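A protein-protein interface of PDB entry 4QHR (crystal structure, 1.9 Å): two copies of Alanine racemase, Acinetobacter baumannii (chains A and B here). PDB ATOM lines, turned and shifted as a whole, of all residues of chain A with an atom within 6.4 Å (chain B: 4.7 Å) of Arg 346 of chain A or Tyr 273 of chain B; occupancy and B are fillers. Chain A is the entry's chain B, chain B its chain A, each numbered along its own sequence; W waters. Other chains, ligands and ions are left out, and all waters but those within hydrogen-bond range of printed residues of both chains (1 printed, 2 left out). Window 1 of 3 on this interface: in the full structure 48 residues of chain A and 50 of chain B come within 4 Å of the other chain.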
ATOM      1  N   TYR A  38      18.797 -23.008  35.099  1.00  0.00           N
ATOM      2  CA  TYR A  38      17.378 -22.774  34.803  1.00  0.00           C
ATOM      3  C   TYR A  38      17.239 -21.462  34.021  1.00  0.00           C
ATOM      4  O   TYR A  38      16.338 -20.687  34.250  1.00  0.00           O
ATOM      5  CB  TYR A  38      16.527 -22.758  36.102  1.00  0.00           C
ATOM      6  CG  TYR A  38      16.256 -24.102  36.797  1.00  0.00           C
ATOM      7  CD1 TYR A  38      17.193 -25.140  36.825  1.00  0.00           C
ATOM      8  CD2 TYR A  38      15.034 -24.316  37.451  1.00  0.00           C
ATOM      9  CE1 TYR A  38      16.923 -26.333  37.489  1.00  0.00           C
ATOM     10  CE2 TYR A  38      14.752 -25.492  38.076  1.00  0.00           C
ATOM     11  CZ  TYR A  38      15.669 -26.493  38.097  1.00  0.00           C
ATOM     12  OH  TYR A  38      15.359 -27.614  38.723  1.00  0.00           O
ATOM     13  N   GLY A  39      18.161 -21.207  33.086  1.00  0.00           N
ATOM     14  CA  GLY A  39      18.094 -19.986  32.272  1.00  0.00           C
ATOM     15  C   GLY A  39      18.773 -18.737  32.850  1.00  0.00           C
ATOM     16  O   GLY A  39      18.913 -17.726  32.160  1.00  0.00           O
ATOM     17  N   TYR A 273       8.713 -12.708  21.105  1.00  0.00           N
ATOM     18  CA  TYR A 273       9.058 -14.131  21.232  1.00  0.00           C
ATOM     19  C   TYR A 273      10.438 -14.474  20.679  1.00  0.00           C
ATOM     20  O   TYR A 273      10.986 -15.509  21.047  1.00  0.00           O
ATOM     21  CB  TYR A 273       7.964 -15.081  20.750  1.00  0.00           C
ATOM     22  CG  TYR A 273       7.676 -14.995  19.284  1.00  0.00           C
ATOM     23  CD1 TYR A 273       8.573 -15.538  18.359  1.00  0.00           C
ATOM     24  CD2 TYR A 273       6.510 -14.356  18.797  1.00  0.00           C
ATOM     25  CE1 TYR A 273       8.308 -15.439  16.968  1.00  0.00           C
ATOM     26  CE2 TYR A 273       6.253 -14.268  17.418  1.00  0.00           C
ATOM     27  CZ  TYR A 273       7.149 -14.789  16.526  1.00  0.00           C
ATOM     28  OH  TYR A 273       6.895 -14.690  15.128  1.00  0.00           O
ATOM     29  N   ASP A 275      12.858 -12.815  21.632  1.00  0.00           N
ATOM     30  CA  ASP A 275      13.638 -12.659  22.866  1.00  0.00           C
ATOM     31  C   ASP A 275      13.400 -13.754  23.907  1.00  0.00           C
ATOM     32  O   ASP A 275      14.162 -13.883  24.863  1.00  0.00           O
ATOM     33  CB  ASP A 275      13.305 -11.319  23.499  1.00  0.00           C
ATOM     34  CG  ASP A 275      13.626 -10.199  22.585  1.00  0.00           C
ATOM     35  OD1 ASP A 275      14.837  -9.914  22.432  1.00  0.00           O
ATOM     36  OD2 ASP A 275      12.650  -9.646  21.991  1.00  0.00           O
ATOM     37  N   GLY A 276      12.364 -14.537  23.687  1.00  0.00           N
ATOM     38  CA  GLY A 276      11.920 -15.534  24.621  1.00  0.00           C
ATOM     39  C   GLY A 276      10.688 -15.081  25.392  1.00  0.00           C
ATOM     40  O   GLY A 276      10.276 -15.796  26.243  1.00  0.00           O
ATOM     41  N   TYR A 277      10.111 -13.905  25.101  1.00  0.00           N
ATOM     42  CA  TYR A 277       8.827 -13.519  25.690  1.00  0.00           C
ATOM     43  C   TYR A 277       7.705 -14.341  25.047  1.00  0.00           C
ATOM     44  O   TYR A 277       7.564 -14.331  23.841  1.00  0.00           O
ATOM     45  CB  TYR A 277       8.561 -12.014  25.522  1.00  0.00           C
ATOM     46  CG  TYR A 277       7.400 -11.509  26.345  1.00  0.00           C
ATOM     47  CD1 TYR A 277       7.550 -11.255  27.720  1.00  0.00           C
ATOM     48  CD2 TYR A 277       6.182 -11.243  25.795  1.00  0.00           C
ATOM     49  CE1 TYR A 277       6.510 -10.793  28.490  1.00  0.00           C
ATOM     50  CE2 TYR A 277       5.132 -10.778  26.579  1.00  0.00           C
ATOM     51  CZ  TYR A 277       5.319 -10.553  27.927  1.00  0.00           C
ATOM     52  OH  TYR A 277       4.301 -10.063  28.727  1.00  0.00           O
ATOM     53  N   ILE A 339       4.193 -23.205  33.211  1.00  0.00           N
ATOM     54  CA  ILE A 339       4.756 -22.950  34.526  1.00  0.00           C
ATOM     55  C   ILE A 339       6.074 -22.133  34.387  1.00  0.00           C
ATOM     56  O   ILE A 339       6.724 -22.122  33.330  1.00  0.00           O
ATOM     57  CB  ILE A 339       4.992 -24.287  35.295  1.00  0.00           C
ATOM     58  CG1 ILE A 339       5.983 -25.179  34.575  1.00  0.00           C
ATOM     59  CG2 ILE A 339       3.639 -24.945  35.602  1.00  0.00           C
ATOM     60  CD1 ILE A 339       6.288 -26.469  35.325  1.00  0.00           C
ATOM     61  N   TYR A 341       9.174 -22.383  35.393  1.00  0.00           N
ATOM     62  CA  TYR A 341      10.300 -23.128  34.940  1.00  0.00           C
ATOM     63  C   TYR A 341      10.541 -22.967  33.435  1.00  0.00           C
ATOM     64  O   TYR A 341      11.662 -22.749  32.994  1.00  0.00           O
ATOM     65  CB  TYR A 341      10.074 -24.640  35.151  1.00  0.00           C
ATOM     66  CG  TYR A 341       9.958 -25.282  36.535  1.00  0.00           C
ATOM     67  CD1 TYR A 341       8.775 -25.202  37.301  1.00  0.00           C
ATOM     68  CD2 TYR A 341      11.005 -26.092  37.041  1.00  0.00           C
ATOM     69  CE1 TYR A 341       8.661 -25.856  38.488  1.00  0.00           C
ATOM     70  CE2 TYR A 341      10.877 -26.746  38.244  1.00  0.00           C
ATOM     71  CZ  TYR A 341       9.678 -26.639  38.949  1.00  0.00           C
ATOM     72  OH  TYR A 341       9.523 -27.272  40.155  1.00  0.00           O
ATOM     73  N   GLU A 342       9.480 -23.112  32.642  1.00  0.00           N
ATOM     74  CA  GLU A 342       9.602 -23.089  31.174  1.00  0.00           C
ATOM     75  C   GLU A 342      10.012 -21.719  30.677  1.00  0.00           C
ATOM     76  O   GLU A 342      10.902 -21.625  29.849  1.00  0.00           O
ATOM     77  CB  GLU A 342       8.345 -23.565  30.460  1.00  0.00           C
ATOM     78  CG  GLU A 342       8.515 -23.581  28.916  1.00  0.00           C
ATOM     79  CD  GLU A 342       7.353 -24.179  28.160  1.00  0.00           C
ATOM     80  OE1 GLU A 342       6.197 -24.170  28.675  1.00  0.00           O
ATOM     81  OE2 GLU A 342       7.573 -24.617  26.995  1.00  0.00           O
ATOM     82  N   LEU A 343       9.372 -20.669  31.173  1.00  0.00           N
ATOM     83  CA  LEU A 343       9.684 -19.289  30.797  1.00  0.00           C
ATOM     84  C   LEU A 343      11.138 -18.904  31.112  1.00  0.00           C
ATOM     85  O   LEU A 343      11.826 -18.243  30.294  1.00  0.00           O
ATOM     86  CB  LEU A 343       8.773 -18.329  31.504  1.00  0.00           C
ATOM     87  CG  LEU A 343       7.404 -18.121  30.927  1.00  0.00           C
ATOM     88  CD1 LEU A 343       6.624 -19.376  30.941  1.00  0.00           C
ATOM     89  CD2 LEU A 343       6.637 -17.020  31.615  1.00  0.00           C
ATOM     90  N   LEU A 344      11.614 -19.397  32.260  1.00  0.00           N
ATOM     91  CA  LEU A 344      12.996 -19.078  32.694  1.00  0.00           C
ATOM     92  C   LEU A 344      14.039 -19.711  31.756  1.00  0.00           C
ATOM     93  O   LEU A 344      15.113 -19.096  31.509  1.00  0.00           O
ATOM     94  CB  LEU A 344      13.197 -19.485  34.165  1.00  0.00           C
ATOM     95  CG  LEU A 344      12.272 -18.717  35.128  1.00  0.00           C
ATOM     96  CD1 LEU A 344      12.115 -19.435  36.454  1.00  0.00           C
ATOM     97  CD2 LEU A 344      12.702 -17.261  35.286  1.00  0.00           C
ATOM     98  N   CYS A 345      13.664 -20.891  31.219  1.00  0.00           N
ATOM     99  CA  CYS A 345      14.497 -21.703  30.332  1.00  0.00           C
ATOM    100  C   CYS A 345      14.527 -21.390  28.829  1.00  0.00           C
ATOM    101  O   CYS A 345      15.446 -21.864  28.131  1.00  0.00           O
ATOM    102  CB  CYS A 345      14.130 -23.190  30.532  1.00  0.00           C
ATOM    103  SG  CYS A 345      14.698 -23.797  32.123  1.00  0.00           S
ATOM    104  N   ARG A 346      13.567 -20.594  28.319  1.00  0.00           N
ATOM    105  CA  ARG A 346      13.397 -20.479  26.870  1.00  0.00           C
ATOM    106  C   ARG A 346      13.506 -19.040  26.359  1.00  0.00           C
ATOM    107  O   ARG A 346      12.807 -18.660  25.428  1.00  0.00           O
ATOM    108  CB  ARG A 346      12.093 -21.178  26.493  1.00  0.00           C
ATOM    109  CG  ARG A 346      12.287 -22.680  26.364  1.00  0.00           C
ATOM    110  CD  ARG A 346      10.960 -23.295  25.942  1.00  0.00           C
ATOM    111  NE  ARG A 346      10.622 -23.011  24.521  1.00  0.00           N
ATOM    112  CZ  ARG A 346       9.388 -22.975  24.016  1.00  0.00           C
ATOM    113  NH1 ARG A 346       8.304 -23.185  24.781  1.00  0.00           N
ATOM    114  NH2 ARG A 346       9.216 -22.698  22.732  1.00  0.00           N
ATOM    115  N   LEU A 347      14.425 -18.283  26.988  1.00  0.00           N
ATOM    116  CA  LEU A 347      14.890 -16.977  26.519  1.00  0.00           C
ATOM    117  C   LEU A 347      15.914 -17.168  25.427  1.00  0.00           C
ATOM    118  O   LEU A 347      16.671 -18.154  25.452  1.00  0.00           O
ATOM    119  CB  LEU A 347      15.489 -16.148  27.666  1.00  0.00           C
ATOM    120  CG  LEU A 347      14.530 -15.887  28.823  1.00  0.00           C
ATOM    121  CD1 LEU A 347      15.291 -15.274  29.978  1.00  0.00           C
ATOM    122  CD2 LEU A 347      13.300 -15.044  28.389  1.00  0.00           C
ATOM    123  N   SER A 348      15.958 -16.232  24.484  1.00  0.00           N
ATOM    124  CA  SER A 348      16.893 -16.312  23.386  1.00  0.00           C
ATOM    125  C   SER A 348      18.207 -15.667  23.822  1.00  0.00           C
ATOM    126  O   SER A 348      18.329 -15.179  24.933  1.00  0.00           O
ATOM    127  CB  SER A 348      16.335 -15.663  22.106  1.00  0.00           C
ATOM    128  OG  SER A 348      16.371 -14.272  22.212  1.00  0.00           O
ATOM    129  N   GLY B 272      14.175 -31.677  26.432  1.00  0.00           N
ATOM    130  CA  GLY B 272      13.045 -31.147  27.192  1.00  0.00           C
ATOM    131  C   GLY B 272      12.963 -29.650  27.024  1.00  0.00           C
ATOM    132  O   GLY B 272      13.624 -29.086  26.127  1.00  0.00           O
ATOM    133  N   TYR B 273      12.212 -28.977  27.886  1.00  0.00           N
ATOM    134  CA  TYR B 273      12.015 -27.560  27.692  1.00  0.00           C
ATOM    135  C   TYR B 273      13.236 -26.758  27.992  1.00  0.00           C
ATOM    136  O   TYR B 273      13.303 -25.630  27.551  1.00  0.00           O
ATOM    137  CB  TYR B 273      10.765 -26.982  28.376  1.00  0.00           C
ATOM    138  CG  TYR B 273      10.798 -27.118  29.885  1.00  0.00           C
ATOM    139  CD1 TYR B 273      11.509 -26.254  30.678  1.00  0.00           C
ATOM    140  CD2 TYR B 273      10.054 -28.128  30.512  1.00  0.00           C
ATOM    141  CE1 TYR B 273      11.513 -26.391  32.079  1.00  0.00           C
ATOM    142  CE2 TYR B 273      10.030 -28.256  31.865  1.00  0.00           C
ATOM    143  CZ  TYR B 273      10.777 -27.424  32.635  1.00  0.00           C
ATOM    144  OH  TYR B 273      10.744 -27.662  34.012  1.00  0.00           O
ATOM    145  N   GLY B 274      14.210 -27.347  28.698  1.00  0.00           N
ATOM    146  CA  GLY B 274      15.519 -26.734  28.910  1.00  0.00           C
ATOM    147  C   GLY B 274      16.368 -26.666  27.665  1.00  0.00           C
ATOM    148  O   GLY B 274      17.382 -25.920  27.639  1.00  0.00           O
ATOM    149  N   ASP B 275      15.985 -27.445  26.644  1.00  0.00           N
ATOM    150  CA  ASP B 275      16.564 -27.318  25.307  1.00  0.00           C
ATOM    151  C   ASP B 275      15.747 -26.440  24.374  1.00  0.00           C
ATOM    152  O   ASP B 275      16.197 -26.127  23.283  1.00  0.00           O
ATOM    153  CB  ASP B 275      16.672 -28.668  24.665  1.00  0.00           C
ATOM    154  CG  ASP B 275      17.430 -29.595  25.489  1.00  0.00           C
ATOM    155  OD1 ASP B 275      18.677 -29.480  25.398  1.00  0.00           O
ATOM    156  OD2 ASP B 275      16.784 -30.381  26.252  1.00  0.00           O
ATOM    157  N   GLY B 276      14.577 -26.050  24.818  1.00  0.00           N
ATOM    158  CA  GLY B 276      13.632 -25.309  23.993  1.00  0.00           C
ATOM    159  C   GLY B 276      12.569 -26.177  23.335  1.00  0.00           C
ATOM    160  O   GLY B 276      11.800 -25.673  22.551  1.00  0.00           O
ATOM    161  N   TYR B 277      12.484 -27.466  23.676  1.00  0.00           N
ATOM    162  CA  TYR B 277      11.344 -28.249  23.250  1.00  0.00           C
ATOM    163  C   TYR B 277      10.120 -27.865  24.108  1.00  0.00           C
ATOM    164  O   TYR B 277      10.251 -27.844  25.326  1.00  0.00           O
ATOM    165  CB  TYR B 277      11.658 -29.729  23.408  1.00  0.00           C
ATOM    166  CG  TYR B 277      10.623 -30.644  22.771  1.00  0.00           C
ATOM    167  CD1 TYR B 277      10.539 -30.779  21.391  1.00  0.00           C
ATOM    168  CD2 TYR B 277       9.744 -31.347  23.531  1.00  0.00           C
ATOM    169  CE1 TYR B 277       9.601 -31.619  20.799  1.00  0.00           C
ATOM    170  CE2 TYR B 277       8.816 -32.218  22.960  1.00  0.00           C
ATOM    171  CZ  TYR B 277       8.735 -32.336  21.591  1.00  0.00           C
ATOM    172  OH  TYR B 277       7.797 -33.198  21.037  1.00  0.00           O
ATOM    173  N   PRO B 278       8.962 -27.525  23.490  1.00  0.00           N
ATOM    174  CA  PRO B 278       7.895 -26.897  24.265  1.00  0.00           C
ATOM    175  C   PRO B 278       7.240 -27.877  25.222  1.00  0.00           C
ATOM    176  O   PRO B 278       7.178 -29.060  24.911  1.00  0.00           O
ATOM    177  CB  PRO B 278       6.876 -26.448  23.218  1.00  0.00           C
ATOM    178  CG  PRO B 278       7.524 -26.580  21.905  1.00  0.00           C
ATOM    179  CD  PRO B 278       8.641 -27.570  22.041  1.00  0.00           C
ATOM    180  N   ARG B 279       6.769 -27.368  26.357  1.00  0.00           N
ATOM    181  CA  ARG B 279       6.267 -28.189  27.439  1.00  0.00           C
ATOM    182  C   ARG B 279       4.790 -28.466  27.325  1.00  0.00           C
ATOM    183  O   ARG B 279       4.376 -29.621  27.543  1.00  0.00           O
ATOM    184  CB  ARG B 279       6.489 -27.481  28.802  1.00  0.00           C
ATOM    185  CG  ARG B 279       5.969 -28.188  30.016  1.00  0.00           C
ATOM    186  CD  ARG B 279       6.262 -27.454  31.336  1.00  0.00           C
ATOM    187  NE  ARG B 279       5.473 -28.059  32.415  1.00  0.00           N
ATOM    188  CZ  ARG B 279       4.191 -27.750  32.691  1.00  0.00           C
ATOM    189  NH1 ARG B 279       3.536 -26.792  32.012  1.00  0.00           N
ATOM    190  NH2 ARG B 279       3.564 -28.356  33.691  1.00  0.00           N
ATOM    191  N   VAL B 300       6.285 -33.118  29.646  1.00  0.00           N
ATOM    192  CA  VAL B 300       7.648 -32.794  29.205  1.00  0.00           C
ATOM    193  C   VAL B 300       8.393 -32.170  30.393  1.00  0.00           C
ATOM    194  O   VAL B 300       7.914 -31.204  30.992  1.00  0.00           O
ATOM    195  CB  VAL B 300       7.580 -31.803  28.007  1.00  0.00           C
ATOM    196  CG1 VAL B 300       8.921 -31.191  27.640  1.00  0.00           C
ATOM    197  CG2 VAL B 300       6.892 -32.467  26.845  1.00  0.00           C
ATOM    198  N   SER B 301       9.569 -32.693  30.715  1.00  0.00           N
ATOM    199  CA  SER B 301      10.348 -32.104  31.815  1.00  0.00           C
ATOM    200  C   SER B 301      11.465 -31.198  31.245  1.00  0.00           C
ATOM    201  O   SER B 301      11.531 -30.962  30.040  1.00  0.00           O
ATOM    202  CB  SER B 301      10.879 -33.226  32.723  1.00  0.00           C
ATOM    203  OG  SER B 301      11.845 -33.997  32.077  1.00  0.00           O
ATOM    204  N   MET B 302      12.299 -30.686  32.130  1.00  0.00           N
ATOM    205  CA  MET B 302      13.346 -29.781  31.702  1.00  0.00           C
ATOM    206  C   MET B 302      14.267 -30.457  30.703  1.00  0.00           C
ATOM    207  O   MET B 302      14.601 -29.840  29.734  1.00  0.00           O
ATOM    208  CB  MET B 302      14.101 -29.217  32.892  1.00  0.00           C
ATOM    209  CG  MET B 302      15.019 -28.043  32.510  1.00  0.00           C
ATOM    210  SD  MET B 302      15.709 -27.254  33.979  1.00  0.00           S
ATOM    211  CE  MET B 302      14.219 -26.533  34.675  1.00  0.00           C
ATOM    212  N   GLU B 342       7.476 -19.325  16.597  1.00  0.00           N
ATOM    213  CA  GLU B 342       7.866 -19.281  18.018  1.00  0.00           C
ATOM    214  C   GLU B 342       8.755 -20.446  18.417  1.00  0.00           C
ATOM    215  O   GLU B 342       9.652 -20.258  19.198  1.00  0.00           O
ATOM    216  CB  GLU B 342       6.647 -19.185  18.949  1.00  0.00           C
ATOM    217  CG  GLU B 342       7.042 -19.129  20.418  1.00  0.00           C
ATOM    218  CD  GLU B 342       5.932 -18.919  21.374  1.00  0.00           C
ATOM    219  OE1 GLU B 342       4.757 -19.335  21.054  1.00  0.00           O
ATOM    220  OE2 GLU B 342       6.229 -18.359  22.455  1.00  0.00           O
ATOM    221  N   LEU B 343       8.514 -21.641  17.876  1.00  0.00           N
ATOM    222  CA  LEU B 343       9.304 -22.832  18.221  1.00  0.00           C
ATOM    223  C   LEU B 343      10.740 -22.657  17.728  1.00  0.00           C
ATOM    224  O   LEU B 343      11.731 -23.004  18.413  1.00  0.00           O
ATOM    225  CB  LEU B 343       8.698 -24.104  17.672  1.00  0.00           C
ATOM    226  CG  LEU B 343       7.615 -24.808  18.488  1.00  0.00           C
ATOM    227  CD1 LEU B 343       6.528 -23.836  18.706  1.00  0.00           C
ATOM    228  CD2 LEU B 343       7.104 -26.065  17.820  1.00  0.00           C
ATOM    229  N   ARG B 346      12.746 -20.062  20.128  1.00  0.00           N
ATOM    230  CA  ARG B 346      12.891 -20.197  21.589  1.00  0.00           C
ATOM    231  C   ARG B 346      13.604 -21.511  22.007  1.00  0.00           C
ATOM    232  O   ARG B 346      13.253 -22.144  22.972  1.00  0.00           O
ATOM    233  CB  ARG B 346      11.546 -20.038  22.226  1.00  0.00           C
ATOM    234  CG  ARG B 346      11.058 -18.555  22.245  1.00  0.00           C
ATOM    235  CD  ARG B 346       9.761 -18.447  22.975  1.00  0.00           C
ATOM    236  NE  ARG B 346       9.840 -18.806  24.422  1.00  0.00           N
ATOM    237  CZ  ARG B 346       8.801 -19.249  25.138  1.00  0.00           C
ATOM    238  NH1 ARG B 346       7.600 -19.430  24.568  1.00  0.00           N
ATOM    239  NH2 ARG B 346       8.924 -19.546  26.435  1.00  0.00           N
HETATM  240  O   HOH W   1      17.281 -23.616  29.144  1.00  0.00           O
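The backbone NH (N) of Arg 279 of chain B lies within hydrogen-bond range of the side-chain carboxylate (OE2) of Glu 342 of chain A (2.9 Å). NE of Arg 346 of chain B sits at hydrogen-bond distance from O of Arg 346 of chain A (3.1 Å).
The backbone NH of Tyr 273 of chain B is in hydrogen-bond range of the backbone carbonyl oxygen of Ser 301 of chain B, 3.0 Å away. The backbone carbonyl oxygen of Met 302 of chain B lies within hydrogen-bond range of the backbone NH of Tyr 273 of chain B (3.1 Å). The backbone carbonyl oxygen (O) of Met 302 of chain B is in hydrogen-bond range of the backbone NH (N) of Gly 274 of chain B. OE2 of Glu 342 of chain B lies within salt-bridge range of NH1 of Arg 346 of chain B (2.7 Å). O of Tyr 341 of chain A lies within hydrogen-bond range of SG of Cys 345 of chain A, 3.3 Å away. NH1 of Arg 346 of chain A lies within salt-bridge range of OE2 of Glu 342 of chain A, 2.7 Å away.
Among the printed residues, pairs that only touch across the chains: Tyr 38 of chain A with Met 302 of chain B (3.6 Å), Tyr 273 of chain A with Glu 342 of chain B (3.8 Å), Tyr 273 of chain A with Arg 346 of chain B (3.3 Å), Gly 276 of chain A with Arg 346 of chain B (3.5 Å), Ile 339 of chain A with Arg 279 of chain B (3.4 Å), Tyr 341 of chain A with Tyr 273 of chain B (3.3 Å), Glu 342 of chain A with Tyr 273 of chain B (3.7 Å), Glu 342 of chain A with Pro 278 of chain B (3.6 Å), Cys 345 of chain A with Tyr 273 of chain B (3.9 Å), Cys 345 of chain A with Met 302 of chain B (3.8 Å), Arg 346 of chain A with Tyr 273 of chain B (3.3 Å), Arg 346 of chain A with Gly 276 of chain B (3.5 Å) and Arg 346 of chain A with Pro 278 of chain B (3.8 Å).
Of the printed residues of chain B, Tyr 273 of chain A touches Glu 342 (3.8 Å) and Arg 346 (3.3 Å). Arg 346 of chain A touches just these residues of chain B: Tyr 273 (3.3 Å), Gly 276 (3.5 Å), Pro 278 (3.8 Å) and Arg 346 (3.1 Å). Gly 272 of chain B touches none of the printed residues of chain A. Printed residues of chain A within 4 Å of Tyr 273 of chain B: Tyr 341 (3.3 Å), Glu 342 (3.7 Å), Cys 345 (3.9 Å) and Arg 346 (3.3 Å). Printed residues of chain A within 4 Å of Gly 276 of chain B: Arg 346 (3.5 Å). The nearest residue of chain B that does not touch Arg 346 of chain A is Glu 342 of chain B (4.3 Å). The nearest residue of chain A that does not touch Tyr 273 of chain B is Ile 339 of chain A (4.8 Å). The nearest printed residue of chain B that does not touch Gly 276 of chain A is Glu 342 of chain B (6.1 Å).
Printed residues of chain B that touch a printed residue of chain A: Tyr 273, Gly 276, Pro 278, Arg 279, Met 302, Glu 342 and Arg 346. Hydrophobic or aromatic side chains of chain B within 4 Å of the printed part of chain A: Tyr 273, Pro 278 and Met 302. Hydrophobic or aromatic side chains of chain A within 4 Å of the printed part of chain B: Tyr 38, Tyr 273, Ile 339 and Tyr 341. Among the printed residues, 15 pairs touch across the chains. Among the printed residues, no Asp or Glu carboxylate lies within 4 Å of a Lys or Arg side-chain nitrogen of the other chain.
Tyr 273 of chain A touches Glu 342 of chain B, and with the chains exchanged Glu 342 of chain A touches Tyr 273 of chain B. Tyr 273 of chain A touches Arg 346 of chain B, and with the chains exchanged Arg 346 of chain A touches Tyr 273 of chain B. Gly 276 of chain A touches Arg 346 of chain B, and with the chains exchanged Arg 346 of chain A touches Gly 276 of chain B. Arg 346 of chain A touches its own counterpart, Arg 346 of chain B. Of the 15 pairs that touch across the chains among the printed residues, 7 have their exchanged pair printed and touching as well.
Water W1 bridges the backbone carbonyl oxygen (O) of Cys 345 of chain A (2.7 Å) and the backbone carbonyl oxygen (O) of Gly 274 of chain B (2.8 Å).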
